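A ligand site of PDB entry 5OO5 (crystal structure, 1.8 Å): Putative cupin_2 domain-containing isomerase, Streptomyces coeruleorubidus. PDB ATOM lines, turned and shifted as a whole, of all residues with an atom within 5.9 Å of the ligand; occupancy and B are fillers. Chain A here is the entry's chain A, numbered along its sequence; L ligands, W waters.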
ATOM      1  N   PHE A  17     -10.783 -16.666   3.240  1.00  0.00           N
ATOM      2  CA  PHE A  17     -10.581 -17.580   4.358  1.00  0.00           C
ATOM      3  C   PHE A  17      -9.934 -16.882   5.536  1.00  0.00           C
ATOM      4  O   PHE A  17      -9.325 -15.818   5.374  1.00  0.00           O
ATOM      5  CB  PHE A  17      -9.733 -18.769   3.908  1.00  0.00           C
ATOM      6  CG  PHE A  17      -8.419 -18.376   3.315  1.00  0.00           C
ATOM      7  CD1 PHE A  17      -8.316 -18.059   1.965  1.00  0.00           C
ATOM      8  CD2 PHE A  17      -7.270 -18.330   4.095  1.00  0.00           C
ATOM      9  CE1 PHE A  17      -7.106 -17.700   1.413  1.00  0.00           C
ATOM     10  CE2 PHE A  17      -6.047 -17.967   3.543  1.00  0.00           C
ATOM     11  CZ  PHE A  17      -5.964 -17.655   2.206  1.00  0.00           C
ATOM     12  N   LYS A  19      -7.082 -16.889   8.423  1.00  0.00           N
ATOM     13  CA  LYS A  19      -5.735 -17.385   8.692  1.00  0.00           C
ATOM     14  C   LYS A  19      -5.209 -16.647   9.906  1.00  0.00           C
ATOM     15  O   LYS A  19      -5.055 -15.421   9.865  1.00  0.00           O
ATOM     16  CB  LYS A  19      -4.843 -17.136   7.475  1.00  0.00           C
ATOM     17  CG  LYS A  19      -3.462 -17.742   7.568  1.00  0.00           C
ATOM     18  CD  LYS A  19      -2.721 -17.633   6.249  1.00  0.00           C
ATOM     19  CE  LYS A  19      -1.339 -18.270   6.325  1.00  0.00           C
ATOM     20  NZ  LYS A  19      -0.598 -18.182   5.030  1.00  0.00           N
ATOM     21  N   HIS A  20      -4.949 -17.369  11.004  1.00  0.00           N
ATOM     22  CA  HIS A  20      -4.388 -16.766  12.223  1.00  0.00           C
ATOM     23  C   HIS A  20      -5.145 -15.525  12.711  1.00  0.00           C
ATOM     24  O   HIS A  20      -4.531 -14.598  13.257  1.00  0.00           O
ATOM     25  CB  HIS A  20      -2.918 -16.393  12.005  1.00  0.00           C
ATOM     26  CG  HIS A  20      -2.067 -17.507  11.512  1.00  0.00           C
ATOM     27  ND1 HIS A  20      -2.015 -18.737  12.144  1.00  0.00           N
ATOM     28  CD2 HIS A  20      -1.221 -17.595  10.459  1.00  0.00           C
ATOM     29  CE1 HIS A  20      -1.185 -19.535  11.493  1.00  0.00           C
ATOM     30  NE2 HIS A  20      -0.690 -18.864  10.466  1.00  0.00           N
ATOM     31  N   ILE A  22      -6.961 -13.337  10.895  1.00  0.00           N
ATOM     32  CA  ILE A  22      -7.304 -12.356   9.843  1.00  0.00           C
ATOM     33  C   ILE A  22      -8.193 -13.005   8.792  1.00  0.00           C
ATOM     34  O   ILE A  22      -8.153 -14.208   8.583  1.00  0.00           O
ATOM     35  CB  ILE A  22      -6.051 -11.711   9.173  1.00  0.00           C
ATOM     36  CG1 ILE A  22      -5.274 -12.712   8.308  1.00  0.00           C
ATOM     37  CG2 ILE A  22      -5.141 -11.086  10.217  1.00  0.00           C
ATOM     38  CD1 ILE A  22      -4.343 -12.070   7.313  1.00  0.00           C
ATOM     39  N   LEU A  24      -8.681 -13.057   4.931  1.00  0.00           N
ATOM     40  CA  LEU A  24      -7.964 -12.751   3.693  1.00  0.00           C
ATOM     41  C   LEU A  24      -8.902 -12.816   2.511  1.00  0.00           C
ATOM     42  O   LEU A  24      -9.775 -13.686   2.455  1.00  0.00           O
ATOM     43  CB  LEU A  24      -6.825 -13.739   3.480  1.00  0.00           C
ATOM     44  CG  LEU A  24      -5.521 -13.396   4.189  1.00  0.00           C
ATOM     45  CD1 LEU A  24      -4.706 -14.646   4.471  1.00  0.00           C
ATOM     46  CD2 LEU A  24      -4.726 -12.392   3.360  1.00  0.00           C
ATOM     47  N   VAL A  26      -8.002 -13.285  -1.280  1.00  0.00           N
ATOM     48  CA  VAL A  26      -6.963 -13.546  -2.260  1.00  0.00           C
ATOM     49  C   VAL A  26      -7.636 -13.564  -3.640  1.00  0.00           C
ATOM     50  O   VAL A  26      -8.373 -14.493  -3.987  1.00  0.00           O
ATOM     51  CB  VAL A  26      -6.240 -14.889  -2.003  1.00  0.00           C
ATOM     52  CG1 VAL A  26      -5.154 -15.131  -3.053  1.00  0.00           C
ATOM     53  CG2 VAL A  26      -5.633 -14.896  -0.608  1.00  0.00           C
ATOM     54  N   THR A  35       2.021  -9.614  -5.716  1.00  0.00           N
ATOM     55  CA  THR A  35       0.627 -10.005  -5.548  1.00  0.00           C
ATOM     56  C   THR A  35      -0.025  -9.101  -4.499  1.00  0.00           C
ATOM     57  O   THR A  35       0.590  -8.732  -3.489  1.00  0.00           O
ATOM     58  CB  THR A  35       0.493 -11.504  -5.190  1.00  0.00           C
ATOM     59  OG1 THR A  35       1.385 -11.827  -4.122  1.00  0.00           O
ATOM     60  CG2 THR A  35       0.859 -12.367  -6.403  1.00  0.00           C
ATOM     61  N   VAL A  37      -3.506  -8.425  -2.075  1.00  0.00           N
ATOM     62  CA  VAL A  37      -4.648  -9.048  -1.420  1.00  0.00           C
ATOM     63  C   VAL A  37      -5.260  -8.072  -0.435  1.00  0.00           C
ATOM     64  O   VAL A  37      -4.653  -7.040  -0.110  1.00  0.00           O
ATOM     65  CB  VAL A  37      -4.245 -10.354  -0.681  1.00  0.00           C
ATOM     66  CG1 VAL A  37      -3.658 -11.367  -1.655  1.00  0.00           C
ATOM     67  CG2 VAL A  37      -3.283 -10.066   0.457  1.00  0.00           C
ATOM     68  N   VAL A  39      -6.850  -7.616   3.488  1.00  0.00           N
ATOM     69  CA  VAL A  39      -6.745  -8.154   4.840  1.00  0.00           C
ATOM     70  C   VAL A  39      -7.733  -7.408   5.718  1.00  0.00           C
ATOM     71  O   VAL A  39      -7.727  -6.180   5.769  1.00  0.00           O
ATOM     72  CB  VAL A  39      -5.322  -7.991   5.420  1.00  0.00           C
ATOM     73  CG1 VAL A  39      -5.270  -8.397   6.883  1.00  0.00           C
ATOM     74  CG2 VAL A  39      -4.325  -8.800   4.599  1.00  0.00           C
ATOM     75  N   HIS A  45      -3.516 -10.606  14.173  1.00  0.00           N
ATOM     76  CA  HIS A  45      -2.883 -11.718  13.470  1.00  0.00           C
ATOM     77  C   HIS A  45      -2.087 -12.482  14.523  1.00  0.00           C
ATOM     78  O   HIS A  45      -0.936 -12.131  14.849  1.00  0.00           O
ATOM     79  CB  HIS A  45      -1.972 -11.187  12.367  1.00  0.00           C
ATOM     80  CG  HIS A  45      -1.380 -12.257  11.511  1.00  0.00           C
ATOM     81  ND1 HIS A  45      -0.324 -13.049  11.919  1.00  0.00           N
ATOM     82  CD2 HIS A  45      -1.722 -12.684  10.272  1.00  0.00           C
ATOM     83  CE1 HIS A  45      -0.041 -13.912  10.965  1.00  0.00           C
ATOM     84  NE2 HIS A  45      -0.869 -13.709   9.948  1.00  0.00           N
ATOM     85  N   GLN A  47      -0.122 -14.865  15.168  1.00  0.00           N
ATOM     86  CA  GLN A  47       0.975 -15.699  14.734  1.00  0.00           C
ATOM     87  C   GLN A  47       2.065 -14.766  14.246  1.00  0.00           C
ATOM     88  O   GLN A  47       1.783 -13.761  13.580  1.00  0.00           O
ATOM     89  CB  GLN A  47       0.540 -16.643  13.590  1.00  0.00           C
ATOM     90  CG  GLN A  47       1.603 -17.657  13.166  1.00  0.00           C
ATOM     91  CD  GLN A  47       2.152 -17.431  11.756  1.00  0.00           C
ATOM     92  OE1 GLN A  47       1.858 -16.434  11.100  1.00  0.00           O
ATOM     93  NE2 GLN A  47       2.940 -18.386  11.277  1.00  0.00           N
ATOM     94  N   PHE A  49       5.511 -14.488  11.986  1.00  0.00           N
ATOM     95  CA  PHE A  49       6.126 -15.153  10.847  1.00  0.00           C
ATOM     96  C   PHE A  49       7.126 -14.208  10.204  1.00  0.00           C
ATOM     97  O   PHE A  49       7.144 -13.008  10.489  1.00  0.00           O
ATOM     98  CB  PHE A  49       5.052 -15.513   9.802  1.00  0.00           C
ATOM     99  CG  PHE A  49       4.415 -14.313   9.157  1.00  0.00           C
ATOM    100  CD1 PHE A  49       3.347 -13.668   9.764  1.00  0.00           C
ATOM    101  CD2 PHE A  49       4.928 -13.792   7.960  1.00  0.00           C
ATOM    102  CE1 PHE A  49       2.786 -12.527   9.186  1.00  0.00           C
ATOM    103  CE2 PHE A  49       4.362 -12.659   7.379  1.00  0.00           C
ATOM    104  CZ  PHE A  49       3.292 -12.031   8.001  1.00  0.00           C
ATOM    105  N   TYR A  56       6.565  -7.064   2.569  1.00  0.00           N
ATOM    106  CA  TYR A  56       5.122  -6.984   2.823  1.00  0.00           C
ATOM    107  C   TYR A  56       4.799  -5.523   3.090  1.00  0.00           C
ATOM    108  O   TYR A  56       5.327  -4.932   4.048  1.00  0.00           O
ATOM    109  CB  TYR A  56       4.702  -7.828   4.031  1.00  0.00           C
ATOM    110  CG  TYR A  56       4.666  -9.334   3.838  1.00  0.00           C
ATOM    111  CD1 TYR A  56       5.706 -10.001   3.169  1.00  0.00           C
ATOM    112  CD2 TYR A  56       3.616 -10.103   4.352  1.00  0.00           C
ATOM    113  CE1 TYR A  56       5.673 -11.384   3.012  1.00  0.00           C
ATOM    114  CE2 TYR A  56       3.597 -11.483   4.194  1.00  0.00           C
ATOM    115  CZ  TYR A  56       4.629 -12.122   3.530  1.00  0.00           C
ATOM    116  OH  TYR A  56       4.622 -13.489   3.387  1.00  0.00           O
ATOM    117  N   TYR A  58       1.715  -2.987   3.847  1.00  0.00           N
ATOM    118  CA  TYR A  58       0.329  -2.856   4.273  1.00  0.00           C
ATOM    119  C   TYR A  58      -0.145  -1.415   4.166  1.00  0.00           C
ATOM    120  O   TYR A  58       0.416  -0.529   4.818  1.00  0.00           O
ATOM    121  CB  TYR A  58       0.165  -3.283   5.731  1.00  0.00           C
ATOM    122  CG  TYR A  58       0.557  -4.693   6.044  1.00  0.00           C
ATOM    123  CD1 TYR A  58       1.887  -5.036   6.222  1.00  0.00           C
ATOM    124  CD2 TYR A  58      -0.404  -5.697   6.215  1.00  0.00           C
ATOM    125  CE1 TYR A  58       2.258  -6.332   6.528  1.00  0.00           C
ATOM    126  CE2 TYR A  58      -0.038  -7.001   6.518  1.00  0.00           C
ATOM    127  CZ  TYR A  58       1.295  -7.307   6.692  1.00  0.00           C
ATOM    128  OH  TYR A  58       1.677  -8.586   7.003  1.00  0.00           O
ATOM    129  N   ILE A  90       7.062 -10.541  11.760  1.00  0.00           N
ATOM    130  CA  ILE A  90       5.845  -9.768  11.667  1.00  0.00           C
ATOM    131  C   ILE A  90       4.744 -10.405  12.500  1.00  0.00           C
ATOM    132  O   ILE A  90       4.450 -11.589  12.355  1.00  0.00           O
ATOM    133  CB  ILE A  90       5.303  -9.722  10.219  1.00  0.00           C
ATOM    134  CG1 ILE A  90       6.285  -8.988   9.292  1.00  0.00           C
ATOM    135  CG2 ILE A  90       3.965  -9.000  10.175  1.00  0.00           C
ATOM    136  CD1 ILE A  90       6.031  -9.280   7.824  1.00  0.00           C
ATOM    137  N   TYR A  92       0.775  -8.515  14.250  1.00  0.00           N
ATOM    138  CA  TYR A  92       0.048  -7.273  14.469  1.00  0.00           C
ATOM    139  C   TYR A  92      -1.245  -7.475  15.221  1.00  0.00           C
ATOM    140  O   TYR A  92      -1.855  -8.548  15.161  1.00  0.00           O
ATOM    141  CB  TYR A  92      -0.209  -6.521  13.169  1.00  0.00           C
ATOM    142  CG  TYR A  92      -0.741  -7.346  12.004  1.00  0.00           C
ATOM    143  CD1 TYR A  92       0.129  -8.057  11.171  1.00  0.00           C
ATOM    144  CD2 TYR A  92      -2.097  -7.363  11.698  1.00  0.00           C
ATOM    145  CE1 TYR A  92      -0.343  -8.791  10.094  1.00  0.00           C
ATOM    146  CE2 TYR A  92      -2.582  -8.101  10.623  1.00  0.00           C
ATOM    147  CZ  TYR A  92      -1.698  -8.805   9.813  1.00  0.00           C
ATOM    148  OH  TYR A  92      -2.169  -9.539   8.736  1.00  0.00           O
ATOM    149  N   LEU A 100      -2.762  -5.370   1.145  1.00  0.00           N
ATOM    150  CA  LEU A 100      -1.412  -5.900   1.327  1.00  0.00           C
ATOM    151  C   LEU A 100      -0.761  -6.249  -0.004  1.00  0.00           C
ATOM    152  O   LEU A 100      -1.324  -7.003  -0.819  1.00  0.00           O
ATOM    153  CB  LEU A 100      -1.456  -7.134   2.219  1.00  0.00           C
ATOM    154  CG  LEU A 100      -0.192  -7.992   2.293  1.00  0.00           C
ATOM    155  CD1 LEU A 100       1.005  -7.228   2.837  1.00  0.00           C
ATOM    156  CD2 LEU A 100      -0.463  -9.197   3.161  1.00  0.00           C
ATOM    157  N   VAL A 102       2.620  -8.045  -1.513  1.00  0.00           N
ATOM    158  CA  VAL A 102       3.787  -8.884  -1.281  1.00  0.00           C
ATOM    159  C   VAL A 102       4.593  -8.886  -2.579  1.00  0.00           C
ATOM    160  O   VAL A 102       4.081  -9.265  -3.641  1.00  0.00           O
ATOM    161  CB  VAL A 102       3.391 -10.304  -0.844  1.00  0.00           C
ATOM    162  CG1 VAL A 102       4.633 -11.167  -0.608  1.00  0.00           C
ATOM    163  CG2 VAL A 102       2.541 -10.240   0.427  1.00  0.00           C
ATOM    164  N   PHE A 106       3.803 -13.378  -3.535  1.00  0.00           N
ATOM    165  CA  PHE A 106       3.691 -14.217  -2.340  1.00  0.00           C
ATOM    166  C   PHE A 106       3.859 -15.687  -2.723  1.00  0.00           C
ATOM    167  O   PHE A 106       3.223 -16.164  -3.668  1.00  0.00           O
ATOM    168  CB  PHE A 106       2.349 -14.009  -1.646  1.00  0.00           C
ATOM    169  CG  PHE A 106       2.079 -14.981  -0.525  1.00  0.00           C
ATOM    170  CD1 PHE A 106       2.594 -14.747   0.738  1.00  0.00           C
ATOM    171  CD2 PHE A 106       1.319 -16.115  -0.740  1.00  0.00           C
ATOM    172  CE1 PHE A 106       2.355 -15.647   1.773  1.00  0.00           C
ATOM    173  CE2 PHE A 106       1.073 -17.018   0.284  1.00  0.00           C
ATOM    174  CZ  PHE A 106       1.601 -16.780   1.546  1.00  0.00           C
ATOM    175  N   GLU A 111       7.652 -18.405   3.456  1.00  0.00           N
ATOM    176  CA  GLU A 111       7.264 -17.929   4.755  1.00  0.00           C
ATOM    177  C   GLU A 111       7.689 -18.930   5.823  1.00  0.00           C
ATOM    178  O   GLU A 111       7.710 -20.148   5.588  1.00  0.00           O
ATOM    179  CB  GLU A 111       5.751 -17.676   4.815  1.00  0.00           C
ATOM    180  CG  GLU A 111       5.407 -16.422   5.578  1.00  0.00           C
ATOM    181  CD  GLU A 111       3.914 -16.230   5.740  1.00  0.00           C
ATOM    182  OE1 GLU A 111       3.329 -16.980   6.554  1.00  0.00           O
ATOM    183  OE2 GLU A 111       3.338 -15.331   5.067  1.00  0.00           O
HETATM  184  N1  LIG L   1      -1.028 -13.966   3.190  1.00  0.00           N
HETATM  185  C1  LIG L   1      -1.031 -14.147   4.642  1.00  0.00           C
HETATM  186  C2  LIG L   1      -0.101 -11.351   6.272  1.00  0.00           C
HETATM  187  C3  LIG L   1      -1.481 -15.002   2.381  1.00  0.00           C
HETATM  188  C4  LIG L   1      -0.978 -13.615   0.419  1.00  0.00           C
HETATM  189  C5  LIG L   1      -0.521 -12.590   1.324  1.00  0.00           C
HETATM  190  O1  LIG L   1      -0.272 -10.502   7.273  1.00  0.00           O
HETATM  191  O2  LIG L   1       0.628 -11.177   5.320  1.00  0.00           O
HETATM  192  C6  LIG L   1      -0.874 -12.657   6.432  1.00  0.00           C
HETATM  193  C7  LIG L   1       0.045 -13.864   6.687  1.00  0.00           C
HETATM  194  O3  LIG L   1      -0.569 -14.863   7.487  1.00  0.00           O
HETATM  195  C8  LIG L   1       0.348 -14.379   5.298  1.00  0.00           C
HETATM  196  O4  LIG L   1       0.768 -15.744   5.215  1.00  0.00           O
HETATM  197  O5  LIG L   1      -1.600 -13.003   5.243  1.00  0.00           O
HETATM  198  O6  LIG L   1      -1.902 -16.075   2.824  1.00  0.00           O
HETATM  199  C9  LIG L   1      -0.558 -12.792   2.648  1.00  0.00           C
HETATM  200  N2  LIG L   1      -1.421 -14.742   1.023  1.00  0.00           N
HETATM  201  O7  LIG L   1      -1.145 -13.470  -0.794  1.00  0.00           O
HETATM  202  O   HOH W   1       1.240 -16.636   8.336  1.00  0.00           O
HETATM  203  O   HOH W   2      -1.960 -18.817   2.602  1.00  0.00           O
HETATM  204  O   HOH W   3      -2.368 -16.991  -0.582  1.00  0.00           O
HETATM  205  O   HOH W   4       0.023 -11.120  -1.805  1.00  0.00           O
HETATM  206  O   HOH W   5      -1.445 -14.750  -3.177  1.00  0.00           O
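An oxygen (O4) of the ligand lies within hydrogen-bond range of the side-chain carboxylate (OE2) of Glu 111 (2.6 Å). The side-chain amino group of Lys 19 is in hydrogen-bond range of an oxygen (O4) of the ligand, at 2.8 Å. NE2 of His 45 lies within hydrogen-bond range of O3 of the ligand (2.7 Å). O1 of the ligand is in hydrogen-bond range of OH of Tyr 92 (2.6 Å). O1 of the ligand is in hydrogen-bond range of OH of Tyr 58, 2.7 Å away.
Water W1 lies within hydrogen-bond range of O3 of the ligand (2.7 Å), OE1 of Glu 111 (2.8 Å) and OE1 of Gln 47 (2.8 Å). Water W2 lies within hydrogen-bond range of an oxygen (O6) of the ligand (2.8 Å) and the side-chain amino group of Lys 19 (2.9 Å). Water W4 bridges OG1 of Thr 35 and O7 of the ligand.
Ile 22 touches the ligand. Leu 24 touches the ligand. Val 37 touches the ligand. Phe 49 touches the ligand. Tyr 56 touches the ligand. Leu 100 touches the ligand (CD2 to O2, 3.1 Å). CG2 of Val 102 touches C5 of the ligand (3.96 Å). CE2 of Phe 106 touches N2 of the ligand, at 3.5 Å. Hydrophobic or aromatic side chains that line the ligand: Ile 22, Leu 24, Val 37, His 45, Phe 49, Tyr 56, Tyr 58, Tyr 92, Leu 100, Val 102 and Phe 106. Within 4 Å of the ligand: Lys 19, Ile 22, Leu 24, Val 37, His 45, Phe 49, Tyr 56, Tyr 58, Tyr 92, Leu 100, Val 102, Phe 106 and Glu 111.
The backbone carbonyl oxygen (O) of Gln 47 sits at hydrogen-bond distance from a ring nitrogen (ND1) of His 45. O of Tyr 92 sits at hydrogen-bond distance from N of His 45, 2.8 Å away. The backbone NH of Val 102 sits at hydrogen-bond distance from the backbone carbonyl oxygen of Thr 35 (2.9 Å). The side-chain hydroxyl (OH) of Tyr 56 lies within hydrogen-bond range of the side-chain carboxylate (OE2) of Glu 111 (2.8 Å). N of Ile 90 lies within hydrogen-bond range of O of Phe 49. The backbone NH (N) of Phe 106 lies within hydrogen-bond range of the side-chain hydroxyl (OG1) of Thr 35 (2.9 Å). O of Val 37 lies within hydrogen-bond range of N of Leu 100 (2.8 Å). N of Leu 24 sits at hydrogen-bond distance from O of Phe 17 (2.9 Å).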
